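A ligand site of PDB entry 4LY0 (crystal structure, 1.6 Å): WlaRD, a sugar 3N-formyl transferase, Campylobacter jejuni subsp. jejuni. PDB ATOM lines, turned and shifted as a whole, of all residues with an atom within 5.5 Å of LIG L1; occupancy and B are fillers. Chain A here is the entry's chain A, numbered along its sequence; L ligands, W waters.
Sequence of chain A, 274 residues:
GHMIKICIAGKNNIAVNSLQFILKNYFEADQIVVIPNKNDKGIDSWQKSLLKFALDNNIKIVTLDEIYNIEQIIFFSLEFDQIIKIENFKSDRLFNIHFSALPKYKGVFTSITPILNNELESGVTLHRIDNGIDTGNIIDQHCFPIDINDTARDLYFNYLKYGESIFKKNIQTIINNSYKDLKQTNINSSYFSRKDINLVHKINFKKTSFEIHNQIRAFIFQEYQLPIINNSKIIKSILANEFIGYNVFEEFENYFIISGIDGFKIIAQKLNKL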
ATOM      1  N   LYS A  11      18.879  24.211  13.226  1.00  0.00           N
ATOM      2  CA  LYS A  11      20.026  25.068  13.607  1.00  0.00           C
ATOM      3  C   LYS A  11      21.093  24.263  14.274  1.00  0.00           C
ATOM      4  O   LYS A  11      20.932  23.113  14.693  1.00  0.00           O
ATOM      5  CB  LYS A  11      19.538  26.233  14.494  1.00  0.00           C
ATOM      6  CG  LYS A  11      19.162  25.761  15.897  1.00  0.00           C
ATOM      7  CD  LYS A  11      18.981  26.945  16.850  1.00  0.00           C
ATOM      8  CE  LYS A  11      18.334  26.537  18.149  1.00  0.00           C
ATOM      9  NZ  LYS A  11      18.252  27.707  19.048  1.00  0.00           N
ATOM     10  N   ASN A  12      22.216  24.975  14.399  1.00  0.00           N
ATOM     11  CA  ASN A  12      23.309  24.637  15.240  1.00  0.00           C
ATOM     12  C   ASN A  12      24.098  23.484  14.666  1.00  0.00           C
ATOM     13  O   ASN A  12      23.829  23.031  13.551  1.00  0.00           O
ATOM     14  CB  ASN A  12      22.848  24.399  16.688  1.00  0.00           C
ATOM     15  CG  ASN A  12      22.531  25.679  17.450  1.00  0.00           C
ATOM     16  OD1 ASN A  12      22.030  25.634  18.619  1.00  0.00           O
ATOM     17  ND2 ASN A  12      22.690  26.810  16.811  1.00  0.00           N
ATOM     18  N   ASN A  37      16.288  28.392  11.160  1.00  0.00           N
ATOM     19  CA  ASN A  37      15.487  29.074  12.163  1.00  0.00           C
ATOM     20  C   ASN A  37      15.404  30.577  11.952  1.00  0.00           C
ATOM     21  O   ASN A  37      16.243  31.175  11.278  1.00  0.00           O
ATOM     22  CB  ASN A  37      15.907  28.736  13.577  1.00  0.00           C
ATOM     23  CG  ASN A  37      15.628  27.310  13.972  1.00  0.00           C
ATOM     24  OD1 ASN A  37      15.065  26.502  13.221  1.00  0.00           O
ATOM     25  ND2 ASN A  37      15.881  27.016  15.218  1.00  0.00           N
ATOM     26  N   SER A  77      13.658  17.667  11.004  1.00  0.00           N
ATOM     27  CA  SER A  77      13.868  18.728  11.996  1.00  0.00           C
ATOM     28  C   SER A  77      15.022  18.406  12.956  1.00  0.00           C
ATOM     29  O   SER A  77      15.052  17.341  13.596  1.00  0.00           O
ATOM     30  CB  SER A  77      12.575  19.004  12.780  1.00  0.00           C
ATOM     31  OG  SER A  77      12.796  19.635  14.011  1.00  0.00           O
ATOM     32  N   LEU A  78      15.965  19.360  12.997  1.00  0.00           N
ATOM     33  CA  LEU A  78      17.150  19.216  13.852  1.00  0.00           C
ATOM     34  C   LEU A  78      17.235  20.566  14.589  1.00  0.00           C
ATOM     35  O   LEU A  78      17.827  21.489  14.069  1.00  0.00           O
ATOM     36  CB  LEU A  78      18.373  18.962  13.011  1.00  0.00           C
ATOM     37  CG  LEU A  78      18.277  17.598  12.258  1.00  0.00           C
ATOM     38  CD1 LEU A  78      19.449  17.433  11.315  1.00  0.00           C
ATOM     39  CD2 LEU A  78      18.214  16.367  13.176  1.00  0.00           C
ATOM     40  N   GLU A  79      16.623  20.652  15.771  1.00  0.00           N
ATOM     41  CA  GLU A  79      16.401  21.869  16.486  1.00  0.00           C
ATOM     42  C   GLU A  79      15.647  22.951  15.743  1.00  0.00           C
ATOM     43  O   GLU A  79      15.901  24.152  15.880  1.00  0.00           O
ATOM     44  CB  GLU A  79      17.726  22.411  17.063  1.00  0.00           C
ATOM     45  CG  GLU A  79      18.339  21.475  18.080  1.00  0.00           C
ATOM     46  CD  GLU A  79      17.382  21.079  19.194  1.00  0.00           C
ATOM     47  OE1 GLU A  79      17.127  21.935  20.076  1.00  0.00           O
ATOM     48  OE2 GLU A  79      16.903  19.914  19.115  1.00  0.00           O
ATOM     49  N   PHE A  80      14.604  22.554  15.027  1.00  0.00           N
ATOM     50  CA  PHE A  80      13.772  23.495  14.317  1.00  0.00           C
ATOM     51  C   PHE A  80      12.823  24.226  15.242  1.00  0.00           C
ATOM     52  O   PHE A  80      12.420  23.654  16.260  1.00  0.00           O
ATOM     53  CB  PHE A  80      12.979  22.683  13.293  1.00  0.00           C
ATOM     54  CG  PHE A  80      12.173  23.492  12.306  1.00  0.00           C
ATOM     55  CD1 PHE A  80      10.886  23.106  11.918  1.00  0.00           C
ATOM     56  CD2 PHE A  80      12.705  24.607  11.685  1.00  0.00           C
ATOM     57  CE1 PHE A  80      10.180  23.796  10.941  1.00  0.00           C
ATOM     58  CE2 PHE A  80      12.009  25.302  10.718  1.00  0.00           C
ATOM     59  CZ  PHE A  80      10.755  24.867  10.301  1.00  0.00           C
ATOM     60  N   ASP A  81      12.502  25.466  14.900  1.00  0.00           N
ATOM     61  CA  ASP A  81      11.756  26.366  15.778  1.00  0.00           C
ATOM     62  C   ASP A  81      10.289  26.490  15.430  1.00  0.00           C
ATOM     63  O   ASP A  81       9.615  27.402  15.914  1.00  0.00           O
ATOM     64  CB  ASP A  81      12.375  27.766  15.817  1.00  0.00           C
ATOM     65  CG  ASP A  81      12.427  28.424  14.447  1.00  0.00           C
ATOM     66  OD1 ASP A  81      12.754  29.648  14.407  1.00  0.00           O
ATOM     67  OD2 ASP A  81      12.072  27.783  13.412  1.00  0.00           O
ATOM     68  N   HIS A  98      14.640  14.826  19.041  1.00  0.00           N
ATOM     69  CA  HIS A  98      14.347  15.530  20.285  1.00  0.00           C
ATOM     70  C   HIS A  98      15.394  15.253  21.373  1.00  0.00           C
ATOM     71  O   HIS A  98      15.869  14.123  21.516  1.00  0.00           O
ATOM     72  CB  HIS A  98      12.978  15.191  20.825  1.00  0.00           C
ATOM     73  CG  HIS A  98      12.627  15.955  22.065  1.00  0.00           C
ATOM     74  ND1 HIS A  98      12.387  17.317  22.109  1.00  0.00           N
ATOM     75  CD2 HIS A  98      12.520  15.522  23.336  1.00  0.00           C
ATOM     76  CE1 HIS A  98      12.097  17.667  23.345  1.00  0.00           C
ATOM     77  NE2 HIS A  98      12.225  16.611  24.122  1.00  0.00           N
ATOM     78  N   GLY A 107       8.996  19.006  25.077  1.00  0.00           N
ATOM     79  CA  GLY A 107       8.980  20.434  25.128  1.00  0.00           C
ATOM     80  C   GLY A 107      10.352  21.053  25.268  1.00  0.00           C
ATOM     81  O   GLY A 107      11.308  20.611  24.662  1.00  0.00           O
ATOM     82  N   VAL A 108      10.445  22.131  26.058  1.00  0.00           N
ATOM     83  CA  VAL A 108      11.552  23.076  25.883  1.00  0.00           C
ATOM     84  C   VAL A 108      12.574  22.927  26.978  1.00  0.00           C
ATOM     85  O   VAL A 108      12.374  22.219  27.982  1.00  0.00           O
ATOM     86  CB  VAL A 108      11.117  24.564  25.959  1.00  0.00           C
ATOM     87  CG1 VAL A 108       9.968  24.873  25.000  1.00  0.00           C
ATOM     88  CG2 VAL A 108      10.593  24.928  27.321  1.00  0.00           C
ATOM     89  N   PHE A 109      13.691  23.594  26.715  1.00  0.00           N
ATOM     90  CA  PHE A 109      14.776  23.714  27.695  1.00  0.00           C
ATOM     91  C   PHE A 109      15.229  22.390  28.315  1.00  0.00           C
ATOM     92  O   PHE A 109      15.412  22.227  29.556  1.00  0.00           O
ATOM     93  CB  PHE A 109      14.375  24.719  28.805  1.00  0.00           C
ATOM     94  CG  PHE A 109      14.210  26.137  28.374  1.00  0.00           C
ATOM     95  CD1 PHE A 109      13.328  26.940  29.077  1.00  0.00           C
ATOM     96  CD2 PHE A 109      14.894  26.690  27.330  1.00  0.00           C
ATOM     97  CE1 PHE A 109      13.126  28.277  28.725  1.00  0.00           C
ATOM     98  CE2 PHE A 109      14.687  28.001  26.964  1.00  0.00           C
ATOM     99  CZ  PHE A 109      13.803  28.794  27.662  1.00  0.00           C
ATOM    100  N   THR A 110      15.485  21.411  27.446  1.00  0.00           N
ATOM    101  CA  THR A 110      15.702  20.078  27.912  1.00  0.00           C
ATOM    102  C   THR A 110      17.141  19.875  28.461  1.00  0.00           C
ATOM    103  O   THR A 110      17.420  18.770  28.952  1.00  0.00           O
ATOM    104  CB  THR A 110      15.477  19.005  26.818  1.00  0.00           C
ATOM    105  OG1 THR A 110      16.345  19.170  25.695  1.00  0.00           O
ATOM    106  CG2 THR A 110      13.996  18.960  26.426  1.00  0.00           C
ATOM    107  N   SER A 111      18.020  20.868  28.302  1.00  0.00           N
ATOM    108  CA  SER A 111      19.300  20.889  29.006  1.00  0.00           C
ATOM    109  C   SER A 111      19.137  21.327  30.461  1.00  0.00           C
ATOM    110  O   SER A 111      20.059  21.122  31.289  1.00  0.00           O
ATOM    111  CB  SER A 111      20.303  21.737  28.235  1.00  0.00           C
ATOM    112  OG  SER A 111      20.507  21.170  26.942  1.00  0.00           O
ATOM    113  N   ILE A 112      17.997  21.915  30.778  1.00  0.00           N
ATOM    114  CA  ILE A 112      17.669  22.430  32.107  1.00  0.00           C
ATOM    115  C   ILE A 112      16.793  21.435  32.846  1.00  0.00           C
ATOM    116  O   ILE A 112      17.060  20.980  33.978  1.00  0.00           O
ATOM    117  CB  ILE A 112      17.019  23.851  32.045  1.00  0.00           C
ATOM    118  CG1 ILE A 112      17.905  24.866  31.308  1.00  0.00           C
ATOM    119  CG2 ILE A 112      16.657  24.287  33.469  1.00  0.00           C
ATOM    120  CD1 ILE A 112      17.390  26.275  31.240  1.00  0.00           C
ATOM    121  N   TYR A 156      23.820  20.110  27.055  1.00  0.00           N
ATOM    122  CA  TYR A 156      23.480  20.569  25.687  1.00  0.00           C
ATOM    123  C   TYR A 156      24.511  20.076  24.654  1.00  0.00           C
ATOM    124  O   TYR A 156      24.169  19.564  23.591  1.00  0.00           O
ATOM    125  CB  TYR A 156      23.306  22.062  25.614  1.00  0.00           C
ATOM    126  CG  TYR A 156      22.764  22.576  24.304  1.00  0.00           C
ATOM    127  CD1 TYR A 156      21.429  22.328  24.019  1.00  0.00           C
ATOM    128  CD2 TYR A 156      23.555  23.108  23.322  1.00  0.00           C
ATOM    129  CE1 TYR A 156      20.896  22.719  22.785  1.00  0.00           C
ATOM    130  CE2 TYR A 156      23.038  23.488  22.058  1.00  0.00           C
ATOM    131  CZ  TYR A 156      21.705  23.259  21.824  1.00  0.00           C
ATOM    132  OH  TYR A 156      21.251  23.660  20.584  1.00  0.00           O
ATOM    133  N   ARG A 194       7.746  27.168  28.055  1.00  0.00           N
ATOM    134  CA  ARG A 194       8.597  28.284  28.450  1.00  0.00           C
ATOM    135  C   ARG A 194       8.102  28.872  29.748  1.00  0.00           C
ATOM    136  O   ARG A 194       8.911  29.123  30.631  1.00  0.00           O
ATOM    137  CB  ARG A 194       8.746  29.302  27.297  1.00  0.00           C
ATOM    138  CG  ARG A 194       9.781  28.842  26.265  1.00  0.00           C
ATOM    139  CD  ARG A 194       9.523  29.201  24.796  1.00  0.00           C
ATOM    140  NE  ARG A 194      10.084  28.255  23.815  1.00  0.00           N
ATOM    141  CZ  ARG A 194       9.794  28.208  22.513  1.00  0.00           C
ATOM    142  NH1 ARG A 194       8.938  29.071  21.978  1.00  0.00           N
ATOM    143  NH2 ARG A 194      10.354  27.286  21.723  1.00  0.00           N
ATOM    144  N   LEU A 199      14.196  31.478  34.076  1.00  0.00           N
ATOM    145  CA  LEU A 199      15.596  31.425  33.781  1.00  0.00           C
ATOM    146  C   LEU A 199      16.406  32.250  34.753  1.00  0.00           C
ATOM    147  O   LEU A 199      17.619  32.107  34.717  1.00  0.00           O
ATOM    148  CB  LEU A 199      15.800  31.955  32.379  1.00  0.00           C
ATOM    149  CG  LEU A 199      15.224  31.026  31.320  1.00  0.00           C
ATOM    150  CD1 LEU A 199      15.133  31.724  29.972  1.00  0.00           C
ATOM    151  CD2 LEU A 199      16.008  29.718  31.250  1.00  0.00           C
ATOM    152  N   PHE A 219      21.159  25.787  35.561  1.00  0.00           N
ATOM    153  CA  PHE A 219      21.119  27.130  35.009  1.00  0.00           C
ATOM    154  C   PHE A 219      22.486  27.602  34.543  1.00  0.00           C
ATOM    155  O   PHE A 219      22.554  28.717  34.053  1.00  0.00           O
ATOM    156  CB  PHE A 219      20.376  28.108  35.889  1.00  0.00           C
ATOM    157  CG  PHE A 219      18.914  27.781  36.036  1.00  0.00           C
ATOM    158  CD1 PHE A 219      18.022  28.302  35.122  1.00  0.00           C
ATOM    159  CD2 PHE A 219      18.437  26.970  37.056  1.00  0.00           C
ATOM    160  CE1 PHE A 219      16.687  27.956  35.211  1.00  0.00           C
ATOM    161  CE2 PHE A 219      17.096  26.654  37.178  1.00  0.00           C
ATOM    162  CZ  PHE A 219      16.240  27.118  36.206  1.00  0.00           C
ATOM    163  N   PHE A 221      24.775  28.038  31.959  1.00  0.00           N
ATOM    164  CA  PHE A 221      24.901  27.984  30.492  1.00  0.00           C
ATOM    165  C   PHE A 221      25.310  29.361  29.989  1.00  0.00           C
ATOM    166  O   PHE A 221      24.489  30.201  29.634  1.00  0.00           O
ATOM    167  CB  PHE A 221      23.597  27.487  29.866  1.00  0.00           C
ATOM    168  CG  PHE A 221      23.740  26.897  28.466  1.00  0.00           C
ATOM    169  CD1 PHE A 221      22.906  25.865  28.060  1.00  0.00           C
ATOM    170  CD2 PHE A 221      24.635  27.428  27.511  1.00  0.00           C
ATOM    171  CE1 PHE A 221      23.031  25.357  26.772  1.00  0.00           C
ATOM    172  CE2 PHE A 221      24.746  26.907  26.232  1.00  0.00           C
ATOM    173  CZ  PHE A 221      23.920  25.850  25.868  1.00  0.00           C
ATOM    174  N   TYR A 224      24.031  32.091  27.687  1.00  0.00           N
ATOM    175  CA  TYR A 224      22.736  32.662  28.051  1.00  0.00           C
ATOM    176  C   TYR A 224      22.707  33.339  29.419  1.00  0.00           C
ATOM    177  O   TYR A 224      22.338  34.511  29.544  1.00  0.00           O
ATOM    178  CB  TYR A 224      21.638  31.595  27.980  1.00  0.00           C
ATOM    179  CG  TYR A 224      21.486  30.964  26.616  1.00  0.00           C
ATOM    180  CD1 TYR A 224      20.778  31.637  25.630  1.00  0.00           C
ATOM    181  CD2 TYR A 224      22.059  29.738  26.280  1.00  0.00           C
ATOM    182  CE1 TYR A 224      20.628  31.090  24.367  1.00  0.00           C
ATOM    183  CE2 TYR A 224      21.936  29.178  25.010  1.00  0.00           C
ATOM    184  CZ  TYR A 224      21.213  29.870  24.058  1.00  0.00           C
ATOM    185  OH  TYR A 224      20.944  29.432  22.766  1.00  0.00           O
ATOM    186  N   GLN A 225      22.996  32.573  30.476  1.00  0.00           N
ATOM    187  CA  GLN A 225      22.972  33.060  31.852  1.00  0.00           C
ATOM    188  C   GLN A 225      23.788  32.157  32.731  1.00  0.00           C
ATOM    189  O   GLN A 225      24.157  31.036  32.384  1.00  0.00           O
ATOM    190  CB  GLN A 225      21.578  33.220  32.417  1.00  0.00           C
ATOM    191  CG  GLN A 225      20.789  32.017  32.868  1.00  0.00           C
ATOM    192  CD  GLN A 225      20.424  31.059  31.740  1.00  0.00           C
ATOM    193  OE1 GLN A 225      19.685  31.445  30.807  1.00  0.00           O
ATOM    194  NE2 GLN A 225      20.899  29.826  31.818  1.00  0.00           N
HETATM  195  O1  LIG L   1      12.267  27.431  19.478  1.00  0.00           O
HETATM  196  C1  LIG L   1      13.645  27.521  19.803  1.00  0.00           C
HETATM  197  C2  LIG L   1      14.057  26.088  20.106  1.00  0.00           C
HETATM  198  O2  LIG L   1      13.208  25.588  21.157  1.00  0.00           O
HETATM  199  C3  LIG L   1      13.982  25.196  18.876  1.00  0.00           C
HETATM  200  O3  LIG L   1      14.815  25.777  17.895  1.00  0.00           O
HETATM  201  C4  LIG L   1      14.468  23.820  19.238  1.00  0.00           C
HETATM  202  O4  LIG L   1      14.186  22.849  18.212  1.00  0.00           O
HETATM  203  C5  LIG L   1      13.669  23.366  20.465  1.00  0.00           C
HETATM  204  O5  LIG L   1      14.198  22.086  20.846  1.00  0.00           O
HETATM  205  C6  LIG L   1      13.729  24.356  21.645  1.00  0.00           C
HETATM  206  O6  LIG L   1      15.093  24.383  22.049  1.00  0.00           O
HETATM  207  P1  LIG L   1      15.350  24.853  23.610  1.00  0.00           P
HETATM  208  O7  LIG L   1      16.523  24.039  24.105  1.00  0.00           O
HETATM  209  O8  LIG L   1      14.076  24.955  24.322  1.00  0.00           O
HETATM  210  O9  LIG L   1      15.718  26.419  23.262  1.00  0.00           O
HETATM  211  P2  LIG L   1      17.049  27.006  22.619  1.00  0.00           P
HETATM  212  O10 LIG L   1      16.620  28.454  22.617  1.00  0.00           O
HETATM  213  O11 LIG L   1      17.648  26.321  21.440  1.00  0.00           O
HETATM  214  O12 LIG L   1      18.167  26.787  23.808  1.00  0.00           O
HETATM  215  C7  LIG L   1      19.050  25.660  23.880  1.00  0.00           C
HETATM  216  C8  LIG L   1      19.462  25.475  25.355  1.00  0.00           C
HETATM  217  O13 LIG L   1      20.086  26.659  25.816  1.00  0.00           O
HETATM  218  C9  LIG L   1      18.299  25.275  26.289  1.00  0.00           C
HETATM  219  O14 LIG L   1      18.018  23.897  26.404  1.00  0.00           O
HETATM  220  C10 LIG L   1      18.850  25.762  27.665  1.00  0.00           C
HETATM  221  C11 LIG L   1      19.718  26.889  27.176  1.00  0.00           C
HETATM  222  N1  LIG L   1      19.152  28.225  27.346  1.00  0.00           N
HETATM  223  C12 LIG L   1      18.413  28.785  26.347  1.00  0.00           C
HETATM  224  C13 LIG L   1      17.893  30.062  26.482  1.00  0.00           C
HETATM  225  C14 LIG L   1      17.138  30.701  25.341  1.00  0.00           C
HETATM  226  C15 LIG L   1      19.357  28.897  28.463  1.00  0.00           C
HETATM  227  O15 LIG L   1      19.994  28.376  29.408  1.00  0.00           O
HETATM  228  N2  LIG L   1      18.879  30.140  28.625  1.00  0.00           N
HETATM  229  C16 LIG L   1      18.187  30.736  27.627  1.00  0.00           C
HETATM  230  O16 LIG L   1      17.746  31.879  27.789  1.00  0.00           O
HETATM  231  N1  LG2 L   2       6.128  19.775  15.121  1.00  0.00           N
HETATM  232  C1  LG2 L   2       5.296  18.839  15.584  1.00  0.00           C
HETATM  233  N2  LG2 L   2       3.979  18.936  15.253  1.00  0.00           N
HETATM  234  N3  LG2 L   2       5.645  17.785  16.341  1.00  0.00           N
HETATM  235  C2  LG2 L   2       6.939  17.690  16.764  1.00  0.00           C
HETATM  236  O1  LG2 L   2       7.209  16.591  17.461  1.00  0.00           O
HETATM  237  C3  LG2 L   2       7.874  18.577  16.268  1.00  0.00           C
HETATM  238  N4  LG2 L   2       9.190  18.498  16.673  1.00  0.00           N
HETATM  239  C4  LG2 L   2       9.902  19.730  16.712  1.00  0.00           C
HETATM  240  C5  LG2 L   2       9.712  20.503  15.411  1.00  0.00           C
HETATM  241  N5  LG2 L   2       8.284  20.575  15.081  1.00  0.00           N
HETATM  242  C6  LG2 L   2       7.428  19.651  15.511  1.00  0.00           C
HETATM  243  C7  LG2 L   2       9.282  20.369  17.940  1.00  0.00           C
HETATM  244  N6  LG2 L   2       9.770  21.688  18.265  1.00  0.00           N
HETATM  245  C8  LG2 L   2       7.512  25.109  19.244  1.00  0.00           C
HETATM  246  C9  LG2 L   2       7.447  23.896  19.913  1.00  0.00           C
HETATM  247  C10 LG2 L   2       8.188  22.780  19.547  1.00  0.00           C
HETATM  248  C11 LG2 L   2       9.009  22.841  18.442  1.00  0.00           C
HETATM  249  C12 LG2 L   2       9.126  24.061  17.782  1.00  0.00           C
HETATM  250  C13 LG2 L   2       8.354  25.186  18.122  1.00  0.00           C
HETATM  251  C14 LG2 L   2       6.625  26.168  19.878  1.00  0.00           C
HETATM  252  N7  LG2 L   2       6.685  26.205  21.244  1.00  0.00           N
HETATM  253  C15 LG2 L   2       5.973  26.966  22.302  1.00  0.00           C
HETATM  254  C16 LG2 L   2       4.702  26.141  22.423  1.00  0.00           C
HETATM  255  C17 LG2 L   2       3.552  26.606  21.517  1.00  0.00           C
HETATM  256  C18 LG2 L   2       2.355  25.754  21.853  1.00  0.00           C
HETATM  257  O2  LG2 L   2       1.859  25.826  22.996  1.00  0.00           O
HETATM  258  O3  LG2 L   2       1.898  24.985  20.988  1.00  0.00           O
HETATM  259  C19 LG2 L   2       6.378  27.179  23.769  1.00  0.00           C
HETATM  260  O4  LG2 L   2       6.276  28.329  24.262  1.00  0.00           O
HETATM  261  O5  LG2 L   2       6.759  26.302  24.590  1.00  0.00           O
HETATM  262  C20 LG2 L   2      11.130  21.866  18.648  1.00  0.00           C
HETATM  263  O6  LG2 L   2      11.907  20.902  18.735  1.00  0.00           O
HETATM  264  O7  LG2 L   2       5.967  26.890  19.125  1.00  0.00           O
HETATM  265  O   HOH W   1      12.570  27.317  23.753  1.00  0.00           O
HETATM  266  O   HOH W   2      15.172  19.008  21.036  1.00  0.00           O
HETATM  267  O   HOH W   3      15.765  33.649  26.695  1.00  0.00           O
HETATM  268  O   HOH W   4      14.955  20.332  23.457  1.00  0.00           O
HETATM  269  O   HOH W   5      12.352  21.161  22.286  1.00  0.00           O
HETATM  270  O   HOH W   6      18.693  23.995  20.423  1.00  0.00           O
HETATM  271  O   HOH W   7      14.200  29.409  23.395  1.00  0.00           O
HETATM  272  O   HOH W   8      18.683  30.298  21.701  1.00  0.00           O
HETATM  273  O   HOH W   9      18.285  21.064  25.162  1.00  0.00           O
HETATM  274  O   HOH W  10      11.669  29.944  18.931  1.00  0.00           O
HETATM  275  O   HOH W  11      18.733  33.893  30.148  1.00  0.00           O
HETATM  276  O   HOH W  12      17.192  21.877  22.795  1.00  0.00           O
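The side-chain amide oxygen (OE1) of Gln 225 sits at hydrogen-bond distance from a nitrogen (N2) of LIG L1, at 2.7 Å.
O4 of LIG L1 is in hydrogen-bond range of N of Phe 80.
The backbone carbonyl oxygen of Phe 80 lies within hydrogen-bond range of an oxygen (O4) of LIG L1.
N of Phe 109 lies within hydrogen-bond range of O8 of LIG L1.
The backbone carbonyl oxygen (O) of Glu 79 is in hydrogen-bond range of an oxygen (O3) of LIG L1.
The side-chain carboxylate of Glu 79 sits at hydrogen-bond distance from an oxygen (O5) of LIG L1 (3.0 Å).
The side-chain amino group of Lys 11 lies within salt-bridge range of an oxygen (O11) of LIG L1, 2.8 Å away.
The guanidinium group of Arg 194 is in hydrogen-bond range of an oxygen (O1) of LIG L1.
ND2 of Asn 37 sits at hydrogen-bond distance from O3 of LIG L1 (3.1 Å).
An oxygen (O4) of LG2 L2 is in salt-bridge range of the guanidinium group (NH1) of Arg 194, at 3.6 Å.
Residues that only touch LIG L1: Asp 81, Val 108, Thr 110, Ser 111, Ile 112, Tyr 156, Leu 199, Phe 221 and Tyr 224.
Hydrophobic or aromatic side chains within 4 Å of LIG L1: Val 108, Phe 109, Ile 112, Tyr 156, Leu 199, Phe 221 and Tyr 224.
Of the 22 residues printed, 16 come within 4 Å of LIG L1.
The nearest printed residue that does not touch LIG L1 is Gly 107 (5.0 Å).
The backbone carbonyl oxygen of Phe 219 sits at hydrogen-bond distance from the side-chain amide nitrogen of Gln 225 (3.0 Å).
The backbone carbonyl oxygen (O) of Glu 79 is in hydrogen-bond range of the side-chain amide nitrogen (ND2) of Asn 37.
The backbone NH of Lys 11 lies within hydrogen-bond range of the backbone carbonyl oxygen of Leu 78 (3.0 Å).
OD1 of Asn 37 is in hydrogen-bond range of N of Asp 81 (3.2 Å).
The backbone NH (N) of Tyr 156 sits close to the side-chain hydroxyl (OG) of Ser 111 (3.5 Å).
The side-chain hydroxyl of Tyr 156 lies within hydrogen-bond range of the side-chain amide oxygen of Asn 12 (2.9 Å).
O4 of LIG L1 lies within hydrogen-bond range of O6 of LG2 L2 (3.0 Å).
Water W12 lies within hydrogen-bond range of an oxygen (O7) of LIG L1 (2.6 Å) and the side-chain carboxylate of Glu 79 (2.7 Å).
Water W6 lies within hydrogen-bond range of OH of Tyr 156 (2.6 Å), OE1 of Glu 79 (2.6 Å) and O11 of LIG L1 (2.7 Å).
Water W1 lies within hydrogen-bond range of NE of Arg 194 (2.7 Å) and O8 of LIG L1 (2.9 Å).
Water W8 bridges OH of Tyr 224 (2.6 Å) and O10 of LIG L1 (2.9 Å).
Water W9 lies within hydrogen-bond range of the side-chain hydroxyl (OG1) of Thr 110, the side-chain hydroxyl (OG) of Ser 111 and an oxygen (O14) of LIG L1.
Water W11 lies within hydrogen-bond range of the side-chain amide oxygen of Gln 225 and an oxygen (O16) of LIG L1.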
